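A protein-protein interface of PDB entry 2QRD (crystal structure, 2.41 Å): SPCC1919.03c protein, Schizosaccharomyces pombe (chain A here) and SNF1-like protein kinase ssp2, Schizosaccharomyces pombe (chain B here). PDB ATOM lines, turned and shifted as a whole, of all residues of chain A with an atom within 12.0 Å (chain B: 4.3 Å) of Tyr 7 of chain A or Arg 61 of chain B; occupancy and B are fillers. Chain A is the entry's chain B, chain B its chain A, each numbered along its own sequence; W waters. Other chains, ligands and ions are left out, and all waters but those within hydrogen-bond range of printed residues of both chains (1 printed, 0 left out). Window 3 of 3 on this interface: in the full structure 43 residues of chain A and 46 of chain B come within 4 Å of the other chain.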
ATOM      1  N   SER A   4     -14.886 -13.449   3.551  1.00  0.00           N
ATOM      2  CA  SER A   4     -14.802 -14.279   4.794  1.00  0.00           C
ATOM      3  C   SER A   4     -13.369 -14.595   5.195  1.00  0.00           C
ATOM      4  O   SER A   4     -12.537 -15.054   4.382  1.00  0.00           O
ATOM      5  CB  SER A   4     -15.633 -15.562   4.696  1.00  0.00           C
ATOM      6  OG  SER A   4     -16.925 -15.318   5.216  1.00  0.00           O
ATOM      7  N   GLU A   5     -13.139 -14.396   6.489  1.00  0.00           N
ATOM      8  CA  GLU A   5     -11.827 -14.114   7.053  1.00  0.00           C
ATOM      9  C   GLU A   5     -11.061 -15.351   7.472  1.00  0.00           C
ATOM     10  O   GLU A   5     -11.633 -16.432   7.638  1.00  0.00           O
ATOM     11  CB  GLU A   5     -11.984 -13.185   8.269  1.00  0.00           C
ATOM     12  CG  GLU A   5     -12.897 -11.997   8.046  1.00  0.00           C
ATOM     13  CD  GLU A   5     -12.252 -10.868   7.252  1.00  0.00           C
ATOM     14  OE1 GLU A   5     -11.044 -10.948   6.906  1.00  0.00           O
ATOM     15  OE2 GLU A   5     -12.971  -9.878   6.980  1.00  0.00           O
ATOM     16  N   GLN A   6      -9.761 -15.153   7.670  1.00  0.00           N
ATOM     17  CA  GLN A   6      -8.856 -16.192   8.142  1.00  0.00           C
ATOM     18  C   GLN A   6      -8.680 -16.069   9.662  1.00  0.00           C
ATOM     19  O   GLN A   6      -7.812 -15.325  10.157  1.00  0.00           O
ATOM     20  CB  GLN A   6      -7.501 -16.071   7.427  1.00  0.00           C
ATOM     21  CG  GLN A   6      -7.571 -16.141   5.901  1.00  0.00           C
ATOM     22  CD  GLN A   6      -7.388 -17.544   5.379  1.00  0.00           C
ATOM     23  OE1 GLN A   6      -7.724 -17.843   4.229  1.00  0.00           O
ATOM     24  NE2 GLN A   6      -6.840 -18.421   6.221  1.00  0.00           N
ATOM     25  N   TYR A   7      -9.506 -16.798  10.404  1.00  0.00           N
ATOM     26  CA  TYR A   7      -9.494 -16.670  11.869  1.00  0.00           C
ATOM     27  C   TYR A   7      -8.412 -17.552  12.485  1.00  0.00           C
ATOM     28  O   TYR A   7      -8.170 -18.675  12.028  1.00  0.00           O
ATOM     29  CB  TYR A   7     -10.869 -16.957  12.475  1.00  0.00           C
ATOM     30  CG  TYR A   7     -11.884 -15.896  12.155  1.00  0.00           C
ATOM     31  CD1 TYR A   7     -12.992 -16.175  11.352  1.00  0.00           C
ATOM     32  CD2 TYR A   7     -11.746 -14.607  12.667  1.00  0.00           C
ATOM     33  CE1 TYR A   7     -13.927 -15.192  11.069  1.00  0.00           C
ATOM     34  CE2 TYR A   7     -12.656 -13.622  12.398  1.00  0.00           C
ATOM     35  CZ  TYR A   7     -13.747 -13.907  11.606  1.00  0.00           C
ATOM     36  OH  TYR A   7     -14.642 -12.893  11.351  1.00  0.00           O
ATOM     37  N   SER A   8      -7.751 -17.013  13.504  1.00  0.00           N
ATOM     38  CA  SER A   8      -6.604 -17.668  14.116  1.00  0.00           C
ATOM     39  C   SER A   8      -6.811 -17.847  15.626  1.00  0.00           C
ATOM     40  O   SER A   8      -7.571 -17.122  16.252  1.00  0.00           O
ATOM     41  CB  SER A   8      -5.338 -16.846  13.810  1.00  0.00           C
ATOM     42  OG  SER A   8      -4.145 -17.540  14.125  1.00  0.00           O
ATOM     43  N   THR A   9      -6.114 -18.816  16.196  1.00  0.00           N
ATOM     44  CA  THR A   9      -6.188 -19.110  17.634  1.00  0.00           C
ATOM     45  C   THR A   9      -4.923 -18.669  18.383  1.00  0.00           C
ATOM     46  O   THR A   9      -4.955 -18.432  19.596  1.00  0.00           O
ATOM     47  CB  THR A   9      -6.467 -20.610  17.886  1.00  0.00           C
ATOM     48  OG1 THR A   9      -6.142 -20.930  19.243  1.00  0.00           O
ATOM     49  CG2 THR A   9      -5.652 -21.501  16.947  1.00  0.00           C
ATOM     50  N   GLU A  10      -3.826 -18.533  17.632  1.00  0.00           N
ATOM     51  CA  GLU A  10      -2.503 -18.250  18.186  1.00  0.00           C
ATOM     52  C   GLU A  10      -2.003 -16.803  17.963  1.00  0.00           C
ATOM     53  O   GLU A  10      -2.133 -16.232  16.865  1.00  0.00           O
ATOM     54  CB  GLU A  10      -1.480 -19.264  17.636  1.00  0.00           C
ATOM     55  CG  GLU A  10      -1.918 -20.741  17.722  1.00  0.00           C
ATOM     56  CD  GLU A  10      -2.109 -21.247  19.158  1.00  0.00           C
ATOM     57  OE1 GLU A  10      -3.256 -21.210  19.663  1.00  0.00           O
ATOM     58  OE2 GLU A  10      -1.114 -21.688  19.778  1.00  0.00           O
ATOM     59  N   ILE A  11      -1.407 -16.239  19.012  1.00  0.00           N
ATOM     60  CA  ILE A  11      -0.857 -14.877  18.985  1.00  0.00           C
ATOM     61  C   ILE A  11       0.268 -14.739  17.926  1.00  0.00           C
ATOM     62  O   ILE A  11       1.129 -15.617  17.811  1.00  0.00           O
ATOM     63  CB  ILE A  11      -0.355 -14.454  20.419  1.00  0.00           C
ATOM     64  CG1 ILE A  11      -1.491 -14.562  21.446  1.00  0.00           C
ATOM     65  CG2 ILE A  11       0.213 -13.029  20.437  1.00  0.00           C
ATOM     66  CD1 ILE A  11      -1.030 -15.088  22.796  1.00  0.00           C
ATOM     67  N   PRO A  12       0.255 -13.639  17.143  1.00  0.00           N
ATOM     68  CA  PRO A  12       1.336 -13.472  16.164  1.00  0.00           C
ATOM     69  C   PRO A  12       2.689 -13.418  16.860  1.00  0.00           C
ATOM     70  O   PRO A  12       2.818 -12.807  17.919  1.00  0.00           O
ATOM     71  CB  PRO A  12       1.015 -12.136  15.488  1.00  0.00           C
ATOM     72  CG  PRO A  12      -0.460 -11.894  15.774  1.00  0.00           C
ATOM     73  CD  PRO A  12      -0.717 -12.522  17.106  1.00  0.00           C
ATOM     74  N   ALA B  39     -11.687 -16.115  22.106  1.00  0.00           N
ATOM     75  CA  ALA B  39     -12.052 -15.583  20.799  1.00  0.00           C
ATOM     76  C   ALA B  39     -11.062 -16.068  19.738  1.00  0.00           C
ATOM     77  O   ALA B  39      -9.966 -16.510  20.067  1.00  0.00           O
ATOM     78  CB  ALA B  39     -12.100 -14.050  20.831  1.00  0.00           C
ATOM     79  N   GLN B  40     -11.473 -16.007  18.475  1.00  0.00           N
ATOM     80  CA  GLN B  40     -10.575 -16.236  17.342  1.00  0.00           C
ATOM     81  C   GLN B  40     -10.519 -14.945  16.573  1.00  0.00           C
ATOM     82  O   GLN B  40     -11.431 -14.152  16.647  1.00  0.00           O
ATOM     83  CB  GLN B  40     -11.063 -17.366  16.447  1.00  0.00           C
ATOM     84  CG  GLN B  40     -10.349 -18.623  16.738  1.00  0.00           C
ATOM     85  CD  GLN B  40     -11.230 -19.856  16.727  1.00  0.00           C
ATOM     86  OE1 GLN B  40     -12.014 -20.084  17.662  1.00  0.00           O
ATOM     87  NE2 GLN B  40     -11.089 -20.665  15.706  1.00  0.00           N
ATOM     88  N   PHE B  41      -9.434 -14.754  15.840  1.00  0.00           N
ATOM     89  CA  PHE B  41      -9.082 -13.441  15.340  1.00  0.00           C
ATOM     90  C   PHE B  41      -8.254 -13.508  14.055  1.00  0.00           C
ATOM     91  O   PHE B  41      -7.564 -14.514  13.768  1.00  0.00           O
ATOM     92  CB  PHE B  41      -8.359 -12.641  16.444  1.00  0.00           C
ATOM     93  CG  PHE B  41      -7.367 -13.466  17.259  1.00  0.00           C
ATOM     94  CD1 PHE B  41      -6.108 -13.773  16.750  1.00  0.00           C
ATOM     95  CD2 PHE B  41      -7.701 -13.946  18.537  1.00  0.00           C
ATOM     96  CE1 PHE B  41      -5.206 -14.515  17.489  1.00  0.00           C
ATOM     97  CE2 PHE B  41      -6.790 -14.697  19.277  1.00  0.00           C
ATOM     98  CZ  PHE B  41      -5.550 -14.978  18.746  1.00  0.00           C
ATOM     99  N   THR B  42      -8.370 -12.459  13.243  1.00  0.00           N
ATOM    100  CA  THR B  42      -7.463 -12.286  12.130  1.00  0.00           C
ATOM    101  C   THR B  42      -6.140 -11.794  12.706  1.00  0.00           C
ATOM    102  O   THR B  42      -6.054 -11.421  13.884  1.00  0.00           O
ATOM    103  CB  THR B  42      -7.962 -11.255  11.113  1.00  0.00           C
ATOM    104  OG1 THR B  42      -8.104  -9.989  11.767  1.00  0.00           O
ATOM    105  CG2 THR B  42      -9.272 -11.698  10.460  1.00  0.00           C
ATOM    106  N   LYS B  59     -10.330  -8.461  13.307  1.00  0.00           N
ATOM    107  CA  LYS B  59     -11.666  -9.052  13.293  1.00  0.00           C
ATOM    108  C   LYS B  59     -11.691 -10.302  14.169  1.00  0.00           C
ATOM    109  O   LYS B  59     -10.844 -11.173  14.050  1.00  0.00           O
ATOM    110  CB  LYS B  59     -12.172  -9.317  11.866  1.00  0.00           C
ATOM    111  CG  LYS B  59     -12.363  -8.035  11.055  1.00  0.00           C
ATOM    112  CD  LYS B  59     -13.434  -8.156  10.029  1.00  0.00           C
ATOM    113  CE  LYS B  59     -13.327  -7.007   9.001  1.00  0.00           C
ATOM    114  NZ  LYS B  59     -14.646  -6.661   8.336  1.00  0.00           N
ATOM    115  N   SER B  60     -12.654 -10.381  15.063  1.00  0.00           N
ATOM    116  CA  SER B  60     -12.672 -11.499  15.994  1.00  0.00           C
ATOM    117  C   SER B  60     -13.998 -12.251  15.896  1.00  0.00           C
ATOM    118  O   SER B  60     -15.053 -11.663  15.605  1.00  0.00           O
ATOM    119  CB  SER B  60     -12.405 -11.031  17.436  1.00  0.00           C
ATOM    120  OG  SER B  60     -13.446 -10.179  17.880  1.00  0.00           O
ATOM    121  N   ARG B  61     -13.927 -13.555  16.095  1.00  0.00           N
ATOM    122  CA  ARG B  61     -15.113 -14.386  16.181  1.00  0.00           C
ATOM    123  C   ARG B  61     -15.171 -15.039  17.563  1.00  0.00           C
ATOM    124  O   ARG B  61     -14.163 -15.555  18.061  1.00  0.00           O
ATOM    125  CB  ARG B  61     -15.112 -15.434  15.072  1.00  0.00           C
ATOM    126  CG  ARG B  61     -16.455 -16.053  14.853  1.00  0.00           C
ATOM    127  CD  ARG B  61     -16.379 -17.097  13.779  1.00  0.00           C
ATOM    128  NE  ARG B  61     -15.344 -18.072  14.090  1.00  0.00           N
ATOM    129  CZ  ARG B  61     -14.804 -18.892  13.206  1.00  0.00           C
ATOM    130  NH1 ARG B  61     -15.227 -18.848  11.949  1.00  0.00           N
ATOM    131  NH2 ARG B  61     -13.845 -19.746  13.580  1.00  0.00           N
ATOM    132  N   TRP B  62     -16.355 -15.007  18.160  1.00  0.00           N
ATOM    133  CA  TRP B  62     -16.591 -15.498  19.522  1.00  0.00           C
ATOM    134  C   TRP B  62     -17.749 -16.490  19.493  1.00  0.00           C
ATOM    135  O   TRP B  62     -18.836 -16.193  18.936  1.00  0.00           O
ATOM    136  CB  TRP B  62     -17.016 -14.346  20.440  1.00  0.00           C
ATOM    137  CG  TRP B  62     -16.059 -13.173  20.596  1.00  0.00           C
ATOM    138  CD1 TRP B  62     -15.660 -12.262  19.632  1.00  0.00           C
ATOM    139  CD2 TRP B  62     -15.440 -12.753  21.809  1.00  0.00           C
ATOM    140  NE1 TRP B  62     -14.799 -11.330  20.180  1.00  0.00           N
ATOM    141  CE2 TRP B  62     -14.659 -11.600  21.514  1.00  0.00           C
ATOM    142  CE3 TRP B  62     -15.456 -13.249  23.120  1.00  0.00           C
ATOM    143  CZ2 TRP B  62     -13.903 -10.939  22.481  1.00  0.00           C
ATOM    144  CZ3 TRP B  62     -14.709 -12.580  24.097  1.00  0.00           C
ATOM    145  CH2 TRP B  62     -13.930 -11.445  23.767  1.00  0.00           C
ATOM    146  N   TYR B  75     -22.367 -17.546  16.516  1.00  0.00           N
ATOM    147  CA  TYR B  75     -21.134 -16.813  16.618  1.00  0.00           C
ATOM    148  C   TYR B  75     -21.431 -15.336  16.635  1.00  0.00           C
ATOM    149  O   TYR B  75     -22.410 -14.890  16.056  1.00  0.00           O
ATOM    150  CB  TYR B  75     -20.254 -17.110  15.395  1.00  0.00           C
ATOM    151  CG  TYR B  75     -19.645 -18.499  15.319  1.00  0.00           C
ATOM    152  CD1 TYR B  75     -20.162 -19.457  14.446  1.00  0.00           C
ATOM    153  CD2 TYR B  75     -18.534 -18.851  16.090  1.00  0.00           C
ATOM    154  CE1 TYR B  75     -19.611 -20.732  14.349  1.00  0.00           C
ATOM    155  CE2 TYR B  75     -17.967 -20.126  15.994  1.00  0.00           C
ATOM    156  CZ  TYR B  75     -18.513 -21.055  15.126  1.00  0.00           C
ATOM    157  OH  TYR B  75     -17.964 -22.312  15.008  1.00  0.00           O
ATOM    158  N   ALA B  76     -20.552 -14.586  17.290  1.00  0.00           N
ATOM    159  CA  ALA B  76     -20.638 -13.154  17.399  1.00  0.00           C
ATOM    160  C   ALA B  76     -19.371 -12.591  16.766  1.00  0.00           C
ATOM    161  O   ALA B  76     -18.281 -13.056  17.052  1.00  0.00           O
ATOM    162  CB  ALA B  76     -20.729 -12.774  18.837  1.00  0.00           C
ATOM    163  N   TYR B  77     -19.526 -11.604  15.891  1.00  0.00           N
ATOM    164  CA  TYR B  77     -18.397 -10.965  15.212  1.00  0.00           C
ATOM    165  C   TYR B  77     -18.119  -9.541  15.739  1.00  0.00           C
ATOM    166  O   TYR B  77     -18.982  -8.652  15.720  1.00  0.00           O
ATOM    167  CB  TYR B  77     -18.644 -10.983  13.722  1.00  0.00           C
ATOM    168  CG  TYR B  77     -18.872 -12.383  13.198  1.00  0.00           C
ATOM    169  CD1 TYR B  77     -17.825 -13.102  12.652  1.00  0.00           C
ATOM    170  CD2 TYR B  77     -20.156 -12.995  13.241  1.00  0.00           C
ATOM    171  CE1 TYR B  77     -18.016 -14.395  12.166  1.00  0.00           C
ATOM    172  CE2 TYR B  77     -20.356 -14.297  12.756  1.00  0.00           C
ATOM    173  CZ  TYR B  77     -19.265 -14.990  12.225  1.00  0.00           C
ATOM    174  OH  TYR B  77     -19.382 -16.264  11.706  1.00  0.00           O
HETATM  175  O   HOH W   1     -15.163 -10.429  12.449  1.00  0.00           O
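O of Phe 41 of chain B sits at hydrogen-bond distance from N of Ser 8 of chain A, at 2.5 Å.
NZ of Lys 59 of chain B is in salt-bridge range of OE2 of Glu 5 of chain A, at 3.9 Å.
Hydrophobic or aromatic side chains of chain B that line the printed part of chain A: Phe 41 and Tyr 77.
Among the printed residues, 14 pairs touch across the chains.
Among the printed residues, Asp or Glu carboxylates within 4 Å of a Lys or Arg side-chain nitrogen of the other chain: Glu 5 of chain A with Lys 59 of chain B (3.9 Å).
The backbone carbonyl oxygen (O) of Gln 40 of chain B is in hydrogen-bond range of the backbone NH (N) of Arg 61 of chain B, at 2.6 Å.
N of Thr 42 of chain B sits at hydrogen-bond distance from O of Lys 59 of chain B (2.9 Å).
NE1 of Trp 62 of chain B lies within hydrogen-bond range of OG of Ser 60 of chain B.
The side-chain carboxylate (OE1) of Glu 10 of chain A is in hydrogen-bond range of the side-chain hydroxyl (OG1) of Thr 9 of chain A.
Among the printed residues, merely in contact across the chains: Glu 5 of chain A with Thr 42 of chain B (3.8 Å), Gln 6 of chain A with Phe 41 of chain B (3.7 Å), Gln 6 of chain A with Thr 42 of chain B (3.6 Å), Tyr 7 of chain A with Gln 40 of chain B (3.998 Å), Tyr 7 of chain A with Phe 41 of chain B (3.4 Å), Tyr 7 of chain A with Lys 59 of chain B (3.5 Å), Tyr 7 of chain A with Ser 60 of chain B (3.99 Å), Tyr 7 of chain A with Arg 61 of chain B (3.5 Å), Tyr 7 of chain A with Tyr 77 of chain B (3.4 Å), Ser 8 of chain A with Gln 40 of chain B (3.2 Å), Thr 9 of chain A with Phe 41 of chain B (3.6 Å) and Glu 10 of chain A with Phe 41 of chain B (3.6 Å).
Of the printed residues of chain B, Tyr 7 of chain A touches Gln 40, Phe 41, Lys 59, Ser 60, Arg 61 and Tyr 77.
Lys 59 of chain B touches just these residues of chain A: Glu 5 and Tyr 7.
No residue of chain A comes within 4 Å of Trp 62 of chain B.
No residue of chain A comes within 4 Å of Ala 76 of chain B.
Of chain A, only Tyr 7 (3.4 Å) comes within 4 Å of Tyr 77 of chain B.
Of the printed residues of chain B, Thr 9 of chain A touches Phe 41.
Printed residues of chain A within 4 Å of Gln 40 of chain B: Tyr 7 (3.998 Å) and Ser 8 (3.2 Å).
Of the printed residues of chain B, Gln 6 of chain A touches Phe 41 and Thr 42.
Ser 4 of chain A touches none of the printed residues of chain B.
Ile 11 of chain A touches none of the printed residues of chain B.
The nearest printed residue of chain B that does not touch Tyr 7 of chain A is Thr 42 of chain B (4.04 Å).
The nearest residue of chain A that does not touch Arg 61 of chain B is Glu 5 of chain A (6.1 Å).
The nearest printed residue of chain A that does not touch Gln 40 of chain B is Thr 9 of chain A (4.3 Å).
Water W1 bridges OH of Tyr 7 of chain A (2.7 Å) and O of Ser 60 of chain B (3.4 Å).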
